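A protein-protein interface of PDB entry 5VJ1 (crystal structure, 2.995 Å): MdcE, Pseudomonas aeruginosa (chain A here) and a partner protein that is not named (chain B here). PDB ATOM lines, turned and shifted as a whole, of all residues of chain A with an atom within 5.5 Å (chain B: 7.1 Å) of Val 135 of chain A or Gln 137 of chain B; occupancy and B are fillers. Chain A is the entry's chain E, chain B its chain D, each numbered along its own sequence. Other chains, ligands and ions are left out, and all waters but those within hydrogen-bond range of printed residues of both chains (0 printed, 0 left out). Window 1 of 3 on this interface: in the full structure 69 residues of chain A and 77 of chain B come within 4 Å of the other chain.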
ATOM      1  N   LEU A 131      17.565  31.784  -4.373  1.00  0.00           N
ATOM      2  CA  LEU A 131      16.700  30.652  -4.072  1.00  0.00           C
ATOM      3  C   LEU A 131      17.498  29.402  -3.710  1.00  0.00           C
ATOM      4  O   LEU A 131      16.953  28.477  -3.129  1.00  0.00           O
ATOM      5  CB  LEU A 131      15.762  30.370  -5.244  1.00  0.00           C
ATOM      6  CG  LEU A 131      14.406  31.099  -5.253  1.00  0.00           C
ATOM      7  CD1 LEU A 131      14.535  32.599  -5.036  1.00  0.00           C
ATOM      8  CD2 LEU A 131      13.683  30.820  -6.560  1.00  0.00           C
ATOM      9  N   ALA A 132      18.778  29.366  -4.066  1.00  0.00           N
ATOM     10  CA  ALA A 132      19.648  28.262  -3.677  1.00  0.00           C
ATOM     11  C   ALA A 132      20.022  28.374  -2.201  1.00  0.00           C
ATOM     12  O   ALA A 132      20.350  27.383  -1.545  1.00  0.00           O
ATOM     13  CB  ALA A 132      20.888  28.239  -4.532  1.00  0.00           C
ATOM     14  N   GLY A 133      20.006  29.598  -1.688  1.00  0.00           N
ATOM     15  CA  GLY A 133      20.290  29.830  -0.281  1.00  0.00           C
ATOM     16  C   GLY A 133      19.126  29.324   0.551  1.00  0.00           C
ATOM     17  O   GLY A 133      19.275  28.820   1.675  1.00  0.00           O
ATOM     18  N   ALA A 134      17.942  29.492  -0.019  1.00  0.00           N
ATOM     19  CA  ALA A 134      16.743  29.000   0.612  1.00  0.00           C
ATOM     20  C   ALA A 134      16.758  27.476   0.656  1.00  0.00           C
ATOM     21  O   ALA A 134      16.644  26.883   1.725  1.00  0.00           O
ATOM     22  CB  ALA A 134      15.517  29.492  -0.129  1.00  0.00           C
ATOM     23  N   VAL A 135      16.949  26.847  -0.497  1.00  0.00           N
ATOM     24  CA  VAL A 135      16.974  25.402  -0.561  1.00  0.00           C
ATOM     25  C   VAL A 135      18.035  24.830   0.359  1.00  0.00           C
ATOM     26  O   VAL A 135      17.733  23.919   1.130  1.00  0.00           O
ATOM     27  CB  VAL A 135      17.175  24.928  -2.006  1.00  0.00           C
ATOM     28  CG1 VAL A 135      17.180  23.420  -2.116  1.00  0.00           C
ATOM     29  CG2 VAL A 135      16.070  25.468  -2.848  1.00  0.00           C
ATOM     30  N   ASP A 136      19.247  25.385   0.324  1.00  0.00           N
ATOM     31  CA  ASP A 136      20.344  24.894   1.177  1.00  0.00           C
ATOM     32  C   ASP A 136      19.962  24.932   2.655  1.00  0.00           C
ATOM     33  O   ASP A 136      20.121  23.944   3.378  1.00  0.00           O
ATOM     34  CB  ASP A 136      21.630  25.698   0.943  1.00  0.00           C
ATOM     35  CG  ASP A 136      22.832  25.122   1.705  1.00  0.00           C
ATOM     36  OD1 ASP A 136      23.081  23.895   1.628  1.00  0.00           O
ATOM     37  OD2 ASP A 136      23.549  25.908   2.369  1.00  0.00           O
ATOM     38  N   ALA A 137      19.458  26.083   3.095  1.00  0.00           N
ATOM     39  CA  ALA A 137      18.987  26.244   4.463  1.00  0.00           C
ATOM     40  C   ALA A 137      18.012  25.127   4.856  1.00  0.00           C
ATOM     41  O   ALA A 137      18.382  24.224   5.617  1.00  0.00           O
ATOM     42  CB  ALA A 137      18.329  27.609   4.627  1.00  0.00           C
ATOM     43  N   TYR A 138      16.800  25.167   4.289  1.00  0.00           N
ATOM     44  CA  TYR A 138      15.760  24.163   4.542  1.00  0.00           C
ATOM     45  C   TYR A 138      16.317  22.759   4.519  1.00  0.00           C
ATOM     46  O   TYR A 138      16.030  21.963   5.398  1.00  0.00           O
ATOM     47  CB  TYR A 138      14.638  24.260   3.513  1.00  0.00           C
ATOM     48  CG  TYR A 138      13.522  25.248   3.798  1.00  0.00           C
ATOM     49  CD1 TYR A 138      12.606  25.037   4.822  1.00  0.00           C
ATOM     50  CD2 TYR A 138      13.363  26.367   3.018  1.00  0.00           C
ATOM     51  CE1 TYR A 138      11.577  25.919   5.048  1.00  0.00           C
ATOM     52  CE2 TYR A 138      12.344  27.253   3.241  1.00  0.00           C
ATOM     53  CZ  TYR A 138      11.456  27.031   4.252  1.00  0.00           C
ATOM     54  OH  TYR A 138      10.449  27.942   4.440  1.00  0.00           O
ATOM     55  N   ALA A 139      17.104  22.458   3.495  1.00  0.00           N
ATOM     56  CA  ALA A 139      17.678  21.136   3.356  1.00  0.00           C
ATOM     57  C   ALA A 139      18.579  20.782   4.542  1.00  0.00           C
ATOM     58  O   ALA A 139      18.434  19.704   5.130  1.00  0.00           O
ATOM     59  CB  ALA A 139      18.437  21.029   2.050  1.00  0.00           C
ATOM     60  N   ARG A 140      19.505  21.674   4.893  1.00  0.00           N
ATOM     61  CA  ARG A 140      20.415  21.409   6.013  1.00  0.00           C
ATOM     62  C   ARG A 140      19.628  21.251   7.313  1.00  0.00           C
ATOM     63  O   ARG A 140      19.994  20.463   8.189  1.00  0.00           O
ATOM     64  CB  ARG A 140      21.471  22.504   6.155  1.00  0.00           C
ATOM     65  CG  ARG A 140      22.427  22.610   4.970  1.00  0.00           C
ATOM     66  CD  ARG A 140      23.734  23.282   5.364  1.00  0.00           C
ATOM     67  NE  ARG A 140      23.495  24.373   6.310  1.00  0.00           N
ATOM     68  CZ  ARG A 140      23.086  25.597   5.982  1.00  0.00           C
ATOM     69  NH1 ARG A 140      22.867  25.924   4.718  1.00  0.00           N
ATOM     70  NH2 ARG A 140      22.898  26.501   6.927  1.00  0.00           N
ATOM     71  N   LEU A 162      10.489  25.243  -5.058  1.00  0.00           N
ATOM     72  CA  LEU A 162      11.725  24.520  -4.785  1.00  0.00           C
ATOM     73  C   LEU A 162      12.382  25.126  -3.551  1.00  0.00           C
ATOM     74  O   LEU A 162      12.983  24.422  -2.730  1.00  0.00           O
ATOM     75  CB  LEU A 162      12.694  24.573  -5.981  1.00  0.00           C
ATOM     76  CG  LEU A 162      12.358  23.652  -7.156  1.00  0.00           C
ATOM     77  CD1 LEU A 162      13.354  23.820  -8.270  1.00  0.00           C
ATOM     78  CD2 LEU A 162      12.268  22.206  -6.724  1.00  0.00           C
ATOM     79  N   ALA A 163      12.245  26.439  -3.427  1.00  0.00           N
ATOM     80  CA  ALA A 163      12.919  27.170  -2.369  1.00  0.00           C
ATOM     81  C   ALA A 163      12.126  27.070  -1.086  1.00  0.00           C
ATOM     82  O   ALA A 163      12.661  26.671  -0.045  1.00  0.00           O
ATOM     83  CB  ALA A 163      13.124  28.630  -2.760  1.00  0.00           C
ATOM     84  N   GLN A 167      11.623  21.034   0.248  1.00  0.00           N
ATOM     85  CA  GLN A 167      12.592  20.322   1.044  1.00  0.00           C
ATOM     86  C   GLN A 167      11.910  19.638   2.218  1.00  0.00           C
ATOM     87  O   GLN A 167      12.580  19.127   3.108  1.00  0.00           O
ATOM     88  CB  GLN A 167      13.697  21.255   1.505  1.00  0.00           C
ATOM     89  CG  GLN A 167      14.656  21.597   0.395  1.00  0.00           C
ATOM     90  CD  GLN A 167      15.198  20.358  -0.286  1.00  0.00           C
ATOM     91  OE1 GLN A 167      15.745  19.469   0.364  1.00  0.00           O
ATOM     92  NE2 GLN A 167      15.037  20.288  -1.608  1.00  0.00           N
ATOM     93  N   ALA B  94      19.363  12.518  -9.558  1.00  0.00           N
ATOM     94  CA  ALA B  94      19.136  12.545  -8.111  1.00  0.00           C
ATOM     95  C   ALA B  94      19.630  11.245  -7.495  1.00  0.00           C
ATOM     96  O   ALA B  94      20.508  11.277  -6.642  1.00  0.00           O
ATOM     97  CB  ALA B  94      17.669  12.782  -7.777  1.00  0.00           C
ATOM     98  N   LEU B  97      23.451  11.032  -7.078  1.00  0.00           N
ATOM     99  CA  LEU B  97      23.951  11.851  -5.986  1.00  0.00           C
ATOM    100  C   LEU B  97      23.583  11.231  -4.625  1.00  0.00           C
ATOM    101  O   LEU B  97      24.277  11.388  -3.626  1.00  0.00           O
ATOM    102  CB  LEU B  97      23.359  13.251  -6.079  1.00  0.00           C
ATOM    103  CG  LEU B  97      23.768  14.049  -7.299  1.00  0.00           C
ATOM    104  CD1 LEU B  97      22.831  15.217  -7.404  1.00  0.00           C
ATOM    105  CD2 LEU B  97      25.169  14.510  -7.182  1.00  0.00           C
ATOM    106  N   LEU B 130       9.960  18.492 -11.919  1.00  0.00           N
ATOM    107  CA  LEU B 130      10.162  19.451 -10.839  1.00  0.00           C
ATOM    108  C   LEU B 130      10.287  18.730  -9.476  1.00  0.00           C
ATOM    109  O   LEU B 130      11.014  19.171  -8.608  1.00  0.00           O
ATOM    110  CB  LEU B 130       9.014  20.464 -10.816  1.00  0.00           C
ATOM    111  CG  LEU B 130       8.899  21.424  -9.633  1.00  0.00           C
ATOM    112  CD1 LEU B 130       9.955  22.530  -9.732  1.00  0.00           C
ATOM    113  CD2 LEU B 130       7.494  21.986  -9.542  1.00  0.00           C
ATOM    114  N   ALA B 132      11.612  15.893  -9.127  1.00  0.00           N
ATOM    115  CA  ALA B 132      12.911  15.269  -9.229  1.00  0.00           C
ATOM    116  C   ALA B 132      14.028  16.246  -8.862  1.00  0.00           C
ATOM    117  O   ALA B 132      14.956  15.905  -8.125  1.00  0.00           O
ATOM    118  CB  ALA B 132      13.112  14.728 -10.638  1.00  0.00           C
ATOM    119  N   ILE B 133      13.940  17.456  -9.399  1.00  0.00           N
ATOM    120  CA  ILE B 133      14.956  18.460  -9.169  1.00  0.00           C
ATOM    121  C   ILE B 133      15.042  18.748  -7.668  1.00  0.00           C
ATOM    122  O   ILE B 133      16.131  18.988  -7.132  1.00  0.00           O
ATOM    123  CB  ILE B 133      14.668  19.728  -9.972  1.00  0.00           C
ATOM    124  CG1 ILE B 133      14.869  19.433 -11.453  1.00  0.00           C
ATOM    125  CG2 ILE B 133      15.594  20.845  -9.554  1.00  0.00           C
ATOM    126  CD1 ILE B 133      14.539  20.575 -12.352  1.00  0.00           C
ATOM    127  N   ALA B 134      13.904  18.713  -6.982  1.00  0.00           N
ATOM    128  CA  ALA B 134      13.907  18.924  -5.540  1.00  0.00           C
ATOM    129  C   ALA B 134      14.694  17.853  -4.852  1.00  0.00           C
ATOM    130  O   ALA B 134      15.293  18.112  -3.825  1.00  0.00           O
ATOM    131  CB  ALA B 134      12.546  18.934  -5.008  1.00  0.00           C
ATOM    132  N   GLU B 135      14.693  16.651  -5.424  1.00  0.00           N
ATOM    133  CA  GLU B 135      15.391  15.508  -4.832  1.00  0.00           C
ATOM    134  C   GLU B 135      16.851  15.518  -5.223  1.00  0.00           C
ATOM    135  O   GLU B 135      17.699  14.953  -4.514  1.00  0.00           O
ATOM    136  CB  GLU B 135      14.737  14.197  -5.246  1.00  0.00           C
ATOM    137  CG  GLU B 135      13.271  14.187  -4.915  1.00  0.00           C
ATOM    138  CD  GLU B 135      12.608  12.894  -5.280  1.00  0.00           C
ATOM    139  OE1 GLU B 135      12.777  12.456  -6.452  1.00  0.00           O
ATOM    140  OE2 GLU B 135      11.909  12.337  -4.398  1.00  0.00           O
ATOM    141  N   ILE B 136      17.108  16.157  -6.368  1.00  0.00           N
ATOM    142  CA  ILE B 136      18.447  16.411  -6.870  1.00  0.00           C
ATOM    143  C   ILE B 136      19.109  17.405  -5.956  1.00  0.00           C
ATOM    144  O   ILE B 136      20.245  17.210  -5.523  1.00  0.00           O
ATOM    145  CB  ILE B 136      18.443  16.989  -8.304  1.00  0.00           C
ATOM    146  CG1 ILE B 136      18.112  15.899  -9.326  1.00  0.00           C
ATOM    147  CG2 ILE B 136      19.787  17.656  -8.629  1.00  0.00           C
ATOM    148  CD1 ILE B 136      18.229  16.349 -10.780  1.00  0.00           C
ATOM    149  N   GLN B 137      18.387  18.484  -5.673  1.00  0.00           N
ATOM    150  CA  GLN B 137      18.849  19.517  -4.753  1.00  0.00           C
ATOM    151  C   GLN B 137      19.124  18.933  -3.362  1.00  0.00           C
ATOM    152  O   GLN B 137      20.223  19.098  -2.817  1.00  0.00           O
ATOM    153  CB  GLN B 137      17.826  20.635  -4.697  1.00  0.00           C
ATOM    154  CG  GLN B 137      17.776  21.428  -5.987  1.00  0.00           C
ATOM    155  CD  GLN B 137      16.733  22.520  -5.953  1.00  0.00           C
ATOM    156  OE1 GLN B 137      15.650  22.340  -5.380  1.00  0.00           O
ATOM    157  NE2 GLN B 137      17.017  23.636  -6.623  1.00  0.00           N
ATOM    158  N   ALA B 138      18.145  18.216  -2.815  1.00  0.00           N
ATOM    159  CA  ALA B 138      18.296  17.592  -1.509  1.00  0.00           C
ATOM    160  C   ALA B 138      19.535  16.716  -1.454  1.00  0.00           C
ATOM    161  O   ALA B 138      20.283  16.746  -0.479  1.00  0.00           O
ATOM    162  CB  ALA B 138      17.072  16.772  -1.173  1.00  0.00           C
ATOM    163  N   ALA B 139      19.771  15.953  -2.510  1.00  0.00           N
ATOM    164  CA  ALA B 139      20.882  15.020  -2.502  1.00  0.00           C
ATOM    165  C   ALA B 139      22.216  15.723  -2.696  1.00  0.00           C
ATOM    166  O   ALA B 139      23.258  15.175  -2.317  1.00  0.00           O
ATOM    167  CB  ALA B 139      20.688  13.967  -3.560  1.00  0.00           C
ATOM    168  N   ILE B 140      22.185  16.920  -3.294  1.00  0.00           N
ATOM    169  CA  ILE B 140      23.403  17.718  -3.502  1.00  0.00           C
ATOM    170  C   ILE B 140      23.867  18.227  -2.143  1.00  0.00           C
ATOM    171  O   ILE B 140      25.040  18.115  -1.803  1.00  0.00           O
ATOM    172  CB  ILE B 140      23.193  18.925  -4.476  1.00  0.00           C
ATOM    173  CG1 ILE B 140      23.281  18.503  -5.929  1.00  0.00           C
ATOM    174  CG2 ILE B 140      24.242  19.996  -4.269  1.00  0.00           C
ATOM    175  CD1 ILE B 140      23.024  19.651  -6.880  1.00  0.00           C
ATOM    176  N   VAL B 141      22.928  18.769  -1.367  1.00  0.00           N
ATOM    177  CA  VAL B 141      23.210  19.229  -0.005  1.00  0.00           C
ATOM    178  C   VAL B 141      23.727  18.086   0.866  1.00  0.00           C
ATOM    179  O   VAL B 141      24.812  18.186   1.451  1.00  0.00           O
ATOM    180  CB  VAL B 141      21.957  19.831   0.672  1.00  0.00           C
ATOM    181  CG1 VAL B 141      22.143  19.891   2.156  1.00  0.00           C
ATOM    182  CG2 VAL B 141      21.631  21.211   0.101  1.00  0.00           C
ATOM    183  N   ASP B 142      22.953  17.005   0.936  1.00  0.00           N
ATOM    184  CA  ASP B 142      23.320  15.829   1.720  1.00  0.00           C
ATOM    185  C   ASP B 142      24.746  15.368   1.377  1.00  0.00           C
ATOM    186  O   ASP B 142      25.525  15.053   2.274  1.00  0.00           O
ATOM    187  CB  ASP B 142      22.270  14.716   1.516  1.00  0.00           C
ATOM    188  CG  ASP B 142      22.665  13.370   2.136  1.00  0.00           C
ATOM    189  OD1 ASP B 142      23.122  13.326   3.284  1.00  0.00           O
ATOM    190  OD2 ASP B 142      22.453  12.330   1.481  1.00  0.00           O
ATOM    191  N   LEU B 143      25.099  15.373   0.095  1.00  0.00           N
ATOM    192  CA  LEU B 143      26.433  14.934  -0.338  1.00  0.00           C
ATOM    193  C   LEU B 143      27.557  15.897   0.039  1.00  0.00           C
ATOM    194  O   LEU B 143      28.649  15.455   0.376  1.00  0.00           O
ATOM    195  CB  LEU B 143      26.459  14.697  -1.850  1.00  0.00           C
ATOM    196  CG  LEU B 143      27.803  14.267  -2.436  1.00  0.00           C
ATOM    197  CD1 LEU B 143      28.316  13.021  -1.728  1.00  0.00           C
ATOM    198  CD2 LEU B 143      27.629  13.986  -3.897  1.00  0.00           C
ATOM    199  N   GLY B 161      16.206  27.346 -15.142  1.00  0.00           N
ATOM    200  CA  GLY B 161      15.106  26.752 -14.401  1.00  0.00           C
ATOM    201  C   GLY B 161      15.534  26.179 -13.064  1.00  0.00           C
ATOM    202  O   GLY B 161      16.439  26.711 -12.413  1.00  0.00           O
ATOM    203  N   GLY B 162      14.878  25.094 -12.657  1.00  0.00           N
ATOM    204  CA  GLY B 162      15.173  24.468 -11.384  1.00  0.00           C
ATOM    205  C   GLY B 162      16.630  24.068 -11.196  1.00  0.00           C
ATOM    206  O   GLY B 162      17.124  24.062 -10.069  1.00  0.00           O
ATOM    207  N   MET B 163      17.328  23.756 -12.287  1.00  0.00           N
ATOM    208  CA  MET B 163      18.720  23.302 -12.192  1.00  0.00           C
ATOM    209  C   MET B 163      19.737  24.444 -12.014  1.00  0.00           C
ATOM    210  O   MET B 163      20.905  24.208 -11.691  1.00  0.00           O
ATOM    211  CB  MET B 163      19.096  22.486 -13.424  1.00  0.00           C
ATOM    212  CG  MET B 163      18.584  21.070 -13.441  1.00  0.00           C
ATOM    213  SD  MET B 163      19.105  20.033 -12.053  1.00  0.00           S
ATOM    214  CE  MET B 163      20.823  19.718 -12.421  1.00  0.00           C
ATOM    215  N   SER B 164      19.300  25.679 -12.229  1.00  0.00           N
ATOM    216  CA  SER B 164      20.153  26.825 -11.949  1.00  0.00           C
ATOM    217  C   SER B 164      20.198  27.008 -10.441  1.00  0.00           C
ATOM    218  O   SER B 164      21.149  27.570  -9.888  1.00  0.00           O
ATOM    219  CB  SER B 164      19.616  28.091 -12.601  1.00  0.00           C
ATOM    220  OG  SER B 164      18.332  28.420 -12.076  1.00  0.00           O
ATOM    221  N   ILE B 165      19.137  26.552  -9.782  1.00  0.00           N
ATOM    222  CA  ILE B 165      19.091  26.617  -8.341  1.00  0.00           C
ATOM    223  C   ILE B 165      19.936  25.460  -7.830  1.00  0.00           C
ATOM    224  O   ILE B 165      20.621  25.571  -6.819  1.00  0.00           O
ATOM    225  CB  ILE B 165      17.661  26.544  -7.799  1.00  0.00           C
ATOM    226  CG1 ILE B 165      16.764  27.568  -8.497  1.00  0.00           C
ATOM    227  CG2 ILE B 165      17.674  26.772  -6.295  1.00  0.00           C
ATOM    228  CD1 ILE B 165      15.344  27.606  -7.971  1.00  0.00           C
ATOM    229  N   ALA B 166      19.931  24.354  -8.555  1.00  0.00           N
ATOM    230  CA  ALA B 166      20.776  23.231  -8.163  1.00  0.00           C
ATOM    231  C   ALA B 166      22.241  23.548  -8.440  1.00  0.00           C
ATOM    232  O   ALA B 166      23.142  23.004  -7.789  1.00  0.00           O
ATOM    233  CB  ALA B 166      20.363  21.957  -8.896  1.00  0.00           C
ATOM    234  N   ALA B 167      22.483  24.432  -9.403  1.00  0.00           N
ATOM    235  CA  ALA B 167      23.849  24.836  -9.702  1.00  0.00           C
ATOM    236  C   ALA B 167      24.364  25.644  -8.533  1.00  0.00           C
ATOM    237  O   ALA B 167      25.466  25.390  -8.054  1.00  0.00           O
ATOM    238  CB  ALA B 167      23.917  25.633 -10.988  1.00  0.00           C
ATOM    239  N   LEU B 169      23.557  25.629  -5.345  1.00  0.00           N
ATOM    240  CA  LEU B 169      23.891  24.746  -4.231  1.00  0.00           C
ATOM    241  C   LEU B 169      25.304  24.126  -4.287  1.00  0.00           C
ATOM    242  O   LEU B 169      25.856  23.701  -3.260  1.00  0.00           O
ATOM    243  CB  LEU B 169      22.868  23.621  -4.147  1.00  0.00           C
ATOM    244  CG  LEU B 169      21.451  24.006  -3.759  1.00  0.00           C
ATOM    245  CD1 LEU B 169      20.617  22.751  -3.766  1.00  0.00           C
ATOM    246  CD2 LEU B 169      21.398  24.626  -2.403  1.00  0.00           C
ATOM    247  N   CYS B 250      25.961  29.706  -0.691  1.00  0.00           N
ATOM    248  CA  CYS B 250      24.675  29.386  -0.067  1.00  0.00           C
ATOM    249  C   CYS B 250      24.522  29.839   1.376  1.00  0.00           C
ATOM    250  O   CYS B 250      23.413  30.161   1.826  1.00  0.00           O
ATOM    251  CB  CYS B 250      24.440  27.892  -0.139  1.00  0.00           C
ATOM    252  SG  CYS B 250      24.159  27.424  -1.799  1.00  0.00           S
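The side-chain amide nitrogen (NE2) of Gln 167 of chain A lies within hydrogen-bond range of the backbone carbonyl oxygen (O) of Ala 134 of chain B.
Of the 13 printed residues of chain A, 9 touch a printed residue of chain B. Hydrophobic or aromatic side chains of chain A within 4 Å of the printed part of chain B: Leu 131, Ala 132, Val 135, Ala 139 and Leu 162. Of the 24 printed residues of chain B, 10 touch a printed residue of chain A. Hydrophobic or aromatic side chains of chain B that line the printed part of chain A: Leu 130, Ile 133, Ala 134, Ala 138, Val 141, Ile 165 and Leu 169. Among the printed residues, 19 pairs touch across the chains. Among the printed residues, no Asp or Glu carboxylate lies within 4 Å of a Lys or Arg side-chain nitrogen of the other chain.
O of Leu 131 of chain A touches CG2 of Ile 165 of chain B, 3.7 Å away. Leu 169 of chain B touches Ala 132 of chain A (CD2 to O, 3.1 Å). Leu 169 of chain B touches Val 135 of chain A. Val 141 of chain B touches Asp 136 of chain A. OD2 of Asp 136 of chain A touches CB of Cys 250 of chain B, at 3.3 Å. Ala 139 of chain A touches Val 141 of chain B (CB to CG2, 3.7 Å). Ile 133 of chain B touches Leu 162 of chain A. CD2 of Leu 162 of chain A touches CB of Ala 134 of chain B (3.7 Å). Leu 162 of chain A touches Gln 137 of chain B. CA of Gly 162 of chain B touches CD1 of Leu 162 of chain A, at 3.7 Å.
The backbone carbonyl oxygen (O) of Gly 162 of chain B sits at hydrogen-bond distance from the side-chain amide nitrogen (NE2) of Gln 137 of chain B. NH1 of Arg 140 of chain A is in salt-bridge range of OD2 of Asp 136 of chain A.
Printed residues of chain B within 4 Å of Val 135 of chain A: Gln 137 and Leu 169. Of the printed residues of chain A, Gln 137 of chain B touches Val 135 (3.8 Å) and Leu 162 (3.6 Å). No residue of chain B comes within 4 Å of Ala 134 of chain A. Printed residues of chain B within 4 Å of Ala 132 of chain A: Ile 165 (3.5 Å), Leu 169 (3.1 Å) and Cys 250 (3.8 Å). Of the printed residues of chain B, Leu 162 of chain A touches Leu 130 (3.7 Å), Ile 133 (3.9 Å), Ala 134 (3.7 Å), Gln 137 (3.6 Å) and Gly 162 (3.7 Å). Of the printed residues of chain A, Ala 138 of chain B touches Gln 167 (3.4 Å). Ile 140 of chain B touches none of the printed residues of chain A. Ala 166 of chain B touches none of the printed residues of chain A. The nearest printed residue of chain B that does not touch Val 135 of chain A is Ile 165 of chain B (4.02 Å). The nearest residue of chain A that does not touch Gln 137 of chain B is Gln 167 of chain A (4.2 Å).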
